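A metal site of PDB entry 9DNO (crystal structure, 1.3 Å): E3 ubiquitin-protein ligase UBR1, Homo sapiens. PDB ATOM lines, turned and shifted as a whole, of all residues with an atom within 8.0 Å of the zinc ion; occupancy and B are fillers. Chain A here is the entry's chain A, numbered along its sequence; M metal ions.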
ATOM      1  N   SER A  20     -23.788 -31.039 -26.403  1.00  0.00           N
ATOM      2  CA  SER A  20     -23.505 -29.656 -26.748  1.00  0.00           C
ATOM      3  C   SER A  20     -23.994 -28.760 -25.640  1.00  0.00           C
ATOM      4  O   SER A  20     -24.835 -29.142 -24.816  1.00  0.00           O
ATOM      5  CB  SER A  20     -24.145 -29.231 -28.066  1.00  0.00           C
ATOM      6  OG  SER A  20     -23.585 -27.998 -28.486  1.00  0.00           O
ATOM      7  N   CYS A  21     -23.438 -27.551 -25.585  1.00  0.00           N
ATOM      8  CA  CYS A  21     -23.926 -26.538 -24.658  1.00  0.00           C
ATOM      9  C   CYS A  21     -24.582 -25.428 -25.450  1.00  0.00           C
ATOM     10  O   CYS A  21     -23.925 -24.735 -26.237  1.00  0.00           O
ATOM     11  CB  CYS A  21     -22.813 -25.996 -23.768  1.00  0.00           C
ATOM     12  SG  CYS A  21     -23.515 -24.793 -22.557  1.00  0.00           S
ATOM     13  N   ARG A  22     -25.885 -25.256 -25.245  1.00  0.00           N
ATOM     14  CA  ARG A  22     -26.615 -24.264 -26.017  1.00  0.00           C
ATOM     15  C   ARG A  22     -26.172 -22.852 -25.645  1.00  0.00           C
ATOM     16  O   ARG A  22     -26.176 -21.959 -26.504  1.00  0.00           O
ATOM     17  CB  ARG A  22     -28.103 -24.439 -25.791  1.00  0.00           C
ATOM     18  CG  ARG A  22     -28.614 -25.820 -26.228  1.00  0.00           C
ATOM     19  CD  ARG A  22     -29.997 -25.977 -25.694  1.00  0.00           C
ATOM     20  NE  ARG A  22     -30.805 -24.863 -26.163  1.00  0.00           N
ATOM     21  CZ  ARG A  22     -31.921 -24.452 -25.564  1.00  0.00           C
ATOM     22  NH1 ARG A  22     -32.349 -25.027 -24.454  1.00  0.00           N
ATOM     23  NH2 ARG A  22     -32.598 -23.444 -26.101  1.00  0.00           N
ATOM     24  N   ASP A  23     -25.752 -22.660 -24.391  1.00  0.00           N
ATOM     25  CA  ASP A  23     -25.266 -21.352 -23.929  1.00  0.00           C
ATOM     26  C   ASP A  23     -23.913 -21.004 -24.548  1.00  0.00           C
ATOM     27  O   ASP A  23     -23.681 -19.852 -24.962  1.00  0.00           O
ATOM     28  CB  ASP A  23     -25.148 -21.364 -22.400  1.00  0.00           C
ATOM     29  CG  ASP A  23     -26.485 -21.593 -21.679  1.00  0.00           C
ATOM     30  OD1 ASP A  23     -27.505 -21.043 -22.131  1.00  0.00           O
ATOM     31  OD2 ASP A  23     -26.495 -22.310 -20.638  1.00  0.00           O
ATOM     32  N   CYS A  24     -22.992 -21.969 -24.611  1.00  0.00           N
ATOM     33  CA  CYS A  24     -21.591 -21.676 -24.871  1.00  0.00           C
ATOM     34  C   CYS A  24     -21.068 -22.086 -26.241  1.00  0.00           C
ATOM     35  O   CYS A  24     -20.040 -21.569 -26.666  1.00  0.00           O
ATOM     36  CB  CYS A  24     -20.704 -22.321 -23.798  1.00  0.00           C
ATOM     37  SG  CYS A  24     -21.134 -21.830 -22.127  1.00  0.00           S
ATOM     38  N   ALA A  25     -21.719 -23.029 -26.934  1.00  0.00           N
ATOM     39  CA  ALA A  25     -21.244 -23.477 -28.229  1.00  0.00           C
ATOM     40  C   ALA A  25     -21.351 -22.348 -29.240  1.00  0.00           C
ATOM     41  O   ALA A  25     -22.370 -21.672 -29.301  1.00  0.00           O
ATOM     42  CB  ALA A  25     -22.116 -24.628 -28.732  1.00  0.00           C
ATOM     43  N   LEU A  32     -19.032 -32.128 -26.942  1.00  0.00           N
ATOM     44  CA  LEU A  32     -18.117 -32.667 -25.941  1.00  0.00           C
ATOM     45  C   LEU A  32     -18.420 -34.150 -25.721  1.00  0.00           C
ATOM     46  O   LEU A  32     -19.577 -34.574 -25.770  1.00  0.00           O
ATOM     47  CB  LEU A  32     -18.312 -31.988 -24.563  1.00  0.00           C
ATOM     48  CG  LEU A  32     -17.995 -30.494 -24.561  1.00  0.00           C
ATOM     49  CD1 LEU A  32     -18.425 -29.864 -23.229  1.00  0.00           C
ATOM     50  CD2 LEU A  32     -16.498 -30.263 -24.777  1.00  0.00           C
ATOM     51  N   PHE A  37     -17.650 -33.334 -20.858  1.00  0.00           N
ATOM     52  CA  PHE A  37     -18.868 -32.665 -20.413  1.00  0.00           C
ATOM     53  C   PHE A  37     -19.018 -32.748 -18.899  1.00  0.00           C
ATOM     54  O   PHE A  37     -19.202 -31.723 -18.231  1.00  0.00           O
ATOM     55  CB  PHE A  37     -20.078 -33.315 -21.096  1.00  0.00           C
ATOM     56  CG  PHE A  37     -21.391 -32.865 -20.521  1.00  0.00           C
ATOM     57  CD1 PHE A  37     -21.873 -31.609 -20.748  1.00  0.00           C
ATOM     58  CD2 PHE A  37     -22.141 -33.729 -19.733  1.00  0.00           C
ATOM     59  CE1 PHE A  37     -23.097 -31.201 -20.202  1.00  0.00           C
ATOM     60  CE2 PHE A  37     -23.342 -33.320 -19.181  1.00  0.00           C
ATOM     61  CZ  PHE A  37     -23.818 -32.072 -19.429  1.00  0.00           C
ATOM     62  N   SER A  40     -16.685 -30.475 -16.863  1.00  0.00           N
ATOM     63  CA  SER A  40     -16.662 -29.107 -17.356  1.00  0.00           C
ATOM     64  C   SER A  40     -17.766 -28.279 -16.718  1.00  0.00           C
ATOM     65  O   SER A  40     -18.689 -28.804 -16.095  1.00  0.00           O
ATOM     66  CB  SER A  40     -16.834 -29.046 -18.894  1.00  0.00           C
ATOM     67  OG  SER A  40     -18.169 -29.304 -19.266  1.00  0.00           O
ATOM     68  N   VAL A  41     -17.643 -26.968 -16.893  1.00  0.00           N
ATOM     69  CA  VAL A  41     -18.658 -26.032 -16.429  1.00  0.00           C
ATOM     70  C   VAL A  41     -20.008 -26.292 -17.085  1.00  0.00           C
ATOM     71  O   VAL A  41     -21.058 -25.940 -16.540  1.00  0.00           O
ATOM     72  CB  VAL A  41     -18.193 -24.587 -16.650  1.00  0.00           C
ATOM     73  CG1 VAL A  41     -18.116 -24.264 -18.136  1.00  0.00           C
ATOM     74  CG2 VAL A  41     -19.134 -23.597 -15.941  1.00  0.00           C
ATOM     75  N   HIS A  42     -19.997 -26.872 -18.303  1.00  0.00           N
ATOM     76  CA  HIS A  42     -21.233 -27.009 -19.068  1.00  0.00           C
ATOM     77  C   HIS A  42     -22.164 -28.047 -18.490  1.00  0.00           C
ATOM     78  O   HIS A  42     -23.322 -28.096 -18.903  1.00  0.00           O
ATOM     79  CB  HIS A  42     -20.914 -27.294 -20.545  1.00  0.00           C
ATOM     80  CG  HIS A  42     -19.854 -26.383 -21.085  1.00  0.00           C
ATOM     81  ND1 HIS A  42     -20.073 -25.055 -21.357  1.00  0.00           N
ATOM     82  CD2 HIS A  42     -18.544 -26.617 -21.343  1.00  0.00           C
ATOM     83  CE1 HIS A  42     -18.946 -24.506 -21.772  1.00  0.00           C
ATOM     84  NE2 HIS A  42     -18.002 -25.437 -21.784  1.00  0.00           N
ATOM     85  N   LYS A  43     -21.693 -28.872 -17.535  1.00  0.00           N
ATOM     86  CA  LYS A  43     -22.587 -29.827 -16.915  1.00  0.00           C
ATOM     87  C   LYS A  43     -23.715 -29.146 -16.169  1.00  0.00           C
ATOM     88  O   LYS A  43     -24.775 -29.747 -15.973  1.00  0.00           O
ATOM     89  CB  LYS A  43     -21.834 -30.781 -15.978  1.00  0.00           C
ATOM     90  CG  LYS A  43     -21.357 -30.195 -14.690  1.00  0.00           C
ATOM     91  CD  LYS A  43     -20.856 -31.297 -13.771  1.00  0.00           C
ATOM     92  CE  LYS A  43     -19.535 -30.965 -13.111  1.00  0.00           C
ATOM     93  NZ  LYS A  43     -18.480 -30.443 -14.043  1.00  0.00           N
ATOM     94  N   ASN A  44     -23.514 -27.895 -15.743  1.00  0.00           N
ATOM     95  CA  ASN A  44     -24.531 -27.103 -15.063  1.00  0.00           C
ATOM     96  C   ASN A  44     -25.181 -26.069 -15.968  1.00  0.00           C
ATOM     97  O   ASN A  44     -25.876 -25.179 -15.480  1.00  0.00           O
ATOM     98  CB  ASN A  44     -23.943 -26.433 -13.807  1.00  0.00           C
ATOM     99  CG  ASN A  44     -23.299 -27.421 -12.867  1.00  0.00           C
ATOM    100  OD1 ASN A  44     -22.118 -27.296 -12.521  1.00  0.00           O
ATOM    101  ND2 ASN A  44     -24.071 -28.415 -12.436  1.00  0.00           N
ATOM    102  N   HIS A  45     -24.992 -26.179 -17.285  1.00  0.00           N
ATOM    103  CA  HIS A  45     -25.567 -25.269 -18.255  1.00  0.00           C
ATOM    104  C   HIS A  45     -26.734 -25.937 -18.974  1.00  0.00           C
ATOM    105  O   HIS A  45     -27.115 -27.072 -18.670  1.00  0.00           O
ATOM    106  CB  HIS A  45     -24.496 -24.830 -19.260  1.00  0.00           C
ATOM    107  CG  HIS A  45     -23.429 -23.966 -18.666  1.00  0.00           C
ATOM    108  ND1 HIS A  45     -22.320 -23.569 -19.373  1.00  0.00           N
ATOM    109  CD2 HIS A  45     -23.298 -23.442 -17.423  1.00  0.00           C
ATOM    110  CE1 HIS A  45     -21.559 -22.815 -18.599  1.00  0.00           C
ATOM    111  NE2 HIS A  45     -22.114 -22.730 -17.411  1.00  0.00           N
ATOM    112  N   ARG A  46     -27.272 -25.250 -19.979  1.00  0.00           N
ATOM    113  CA  ARG A  46     -28.382 -25.781 -20.769  1.00  0.00           C
ATOM    114  C   ARG A  46     -27.830 -26.643 -21.892  1.00  0.00           C
ATOM    115  O   ARG A  46     -27.715 -26.239 -23.048  1.00  0.00           O
ATOM    116  CB  ARG A  46     -29.212 -24.647 -21.350  1.00  0.00           C
ATOM    117  CG  ARG A  46     -29.896 -23.783 -20.317  1.00  0.00           C
ATOM    118  CD  ARG A  46     -30.873 -22.840 -21.009  1.00  0.00           C
ATOM    119  NE  ARG A  46     -30.180 -21.972 -21.952  1.00  0.00           N
ATOM    120  CZ  ARG A  46     -30.753 -21.404 -23.005  1.00  0.00           C
ATOM    121  NH1 ARG A  46     -32.018 -21.626 -23.312  1.00  0.00           N
ATOM    122  NH2 ARG A  46     -30.031 -20.576 -23.762  1.00  0.00           N
ATOM    123  N   TYR A  47     -27.547 -27.884 -21.551  1.00  0.00           N
ATOM    124  CA  TYR A  47     -26.903 -28.774 -22.492  1.00  0.00           C
ATOM    125  C   TYR A  47     -27.937 -29.565 -23.286  1.00  0.00           C
ATOM    126  O   TYR A  47     -29.115 -29.630 -22.934  1.00  0.00           O
ATOM    127  CB  TYR A  47     -25.953 -29.713 -21.744  1.00  0.00           C
ATOM    128  CG  TYR A  47     -26.652 -30.657 -20.789  1.00  0.00           C
ATOM    129  CD1 TYR A  47     -27.097 -31.896 -21.217  1.00  0.00           C
ATOM    130  CD2 TYR A  47     -26.847 -30.309 -19.455  1.00  0.00           C
ATOM    131  CE1 TYR A  47     -27.715 -32.761 -20.339  1.00  0.00           C
ATOM    132  CE2 TYR A  47     -27.474 -31.170 -18.576  1.00  0.00           C
ATOM    133  CZ  TYR A  47     -27.905 -32.399 -19.028  1.00  0.00           C
ATOM    134  OH  TYR A  47     -28.525 -33.267 -18.170  1.00  0.00           O
ATOM    135  N   TRP A  66     -15.905 -22.302 -28.034  1.00  0.00           N
ATOM    136  CA  TRP A  66     -16.684 -22.194 -26.802  1.00  0.00           C
ATOM    137  C   TRP A  66     -16.653 -20.765 -26.291  1.00  0.00           C
ATOM    138  O   TRP A  66     -15.577 -20.192 -26.127  1.00  0.00           O
ATOM    139  CB  TRP A  66     -16.130 -23.138 -25.730  1.00  0.00           C
ATOM    140  CG  TRP A  66     -16.144 -24.564 -26.193  1.00  0.00           C
ATOM    141  CD1 TRP A  66     -15.068 -25.312 -26.602  1.00  0.00           C
ATOM    142  CD2 TRP A  66     -17.296 -25.406 -26.345  1.00  0.00           C
ATOM    143  NE1 TRP A  66     -15.501 -26.580 -26.977  1.00  0.00           N
ATOM    144  CE2 TRP A  66     -16.853 -26.664 -26.798  1.00  0.00           C
ATOM    145  CE3 TRP A  66     -18.661 -25.233 -26.079  1.00  0.00           C
ATOM    146  CZ2 TRP A  66     -17.723 -27.724 -27.057  1.00  0.00           C
ATOM    147  CZ3 TRP A  66     -19.540 -26.288 -26.338  1.00  0.00           C
ATOM    148  CH2 TRP A  66     -19.060 -27.515 -26.821  1.00  0.00           C
ATOM    149  N   LYS A  67     -17.829 -20.197 -26.033  1.00  0.00           N
ATOM    150  CA  LYS A  67     -17.874 -18.819 -25.563  1.00  0.00           C
ATOM    151  C   LYS A  67     -17.437 -18.692 -24.108  1.00  0.00           C
ATOM    152  O   LYS A  67     -16.978 -17.614 -23.700  1.00  0.00           O
ATOM    153  CB  LYS A  67     -19.262 -18.225 -25.806  1.00  0.00           C
ATOM    154  CG  LYS A  67     -19.646 -18.210 -27.271  1.00  0.00           C
ATOM    155  CD  LYS A  67     -20.956 -17.493 -27.504  1.00  0.00           C
ATOM    156  CE  LYS A  67     -22.046 -18.455 -27.885  1.00  0.00           C
ATOM    157  NZ  LYS A  67     -23.048 -17.818 -28.804  1.00  0.00           N
ATOM    158  N   THR A  68     -17.600 -19.756 -23.318  1.00  0.00           N
ATOM    159  CA  THR A  68     -17.016 -19.885 -21.994  1.00  0.00           C
ATOM    160  C   THR A  68     -16.558 -21.325 -21.817  1.00  0.00           C
ATOM    161  O   THR A  68     -17.001 -22.213 -22.553  1.00  0.00           O
ATOM    162  CB  THR A  68     -18.005 -19.562 -20.850  1.00  0.00           C
ATOM    163  OG1 THR A  68     -18.730 -20.754 -20.469  1.00  0.00           O
ATOM    164  CG2 THR A  68     -18.998 -18.485 -21.251  1.00  0.00           C
ATOM    165  N   GLY A  69     -15.695 -21.577 -20.839  1.00  0.00           N
ATOM    166  CA  GLY A  69     -15.277 -22.924 -20.505  1.00  0.00           C
ATOM    167  C   GLY A  69     -14.767 -23.773 -21.664  1.00  0.00           C
ATOM    168  O   GLY A  69     -15.234 -24.897 -21.890  1.00  0.00           O
HETATM  169 ZN    ZN M   1     -21.791 -23.910 -21.360  1.00  0.00          ZN
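A ring nitrogen (NE2) of His 45 lies close to the backbone carbonyl oxygen of Val 41 (3.5 Å).
N of Asp 23 sits close to SG of Cys 21 (3.6 Å).
NE2 of His 42 sits at hydrogen-bond distance from O of Gly 69 (2.8 Å).
O of Cys 24 lies within hydrogen-bond range of N of Lys 67 (2.7 Å).
The side-chain sulfur (SG) of Cys 24 lies close to the side-chain hydroxyl (OG1) of Thr 68 (3.1 Å).
The backbone NH (N) of His 42 sits close to the side-chain hydroxyl (OG) of Ser 40 (3.2 Å).
NE2 of His 42 lies close to O of Thr 68 (3.5 Å).
The zinc ion is bound by a ring nitrogen (ND1) of His 42, 2.1 Å away.
A ring nitrogen (ND1) of His 45 is bound to the zinc ion, 2.1 Å away.
The side-chain sulfur (SG) of Cys 21 binds the zinc ion, 2.3 Å away.
The zinc ion is bound by SG of Cys 24 (2.3 Å).
The zinc ion has four donor atoms within binding distance.
Of the 20 residues printed, 4 come within 4 Å of the zinc ion.
The nearest printed residue that does not touch the zinc ion is Asp 23 (4.3 Å).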
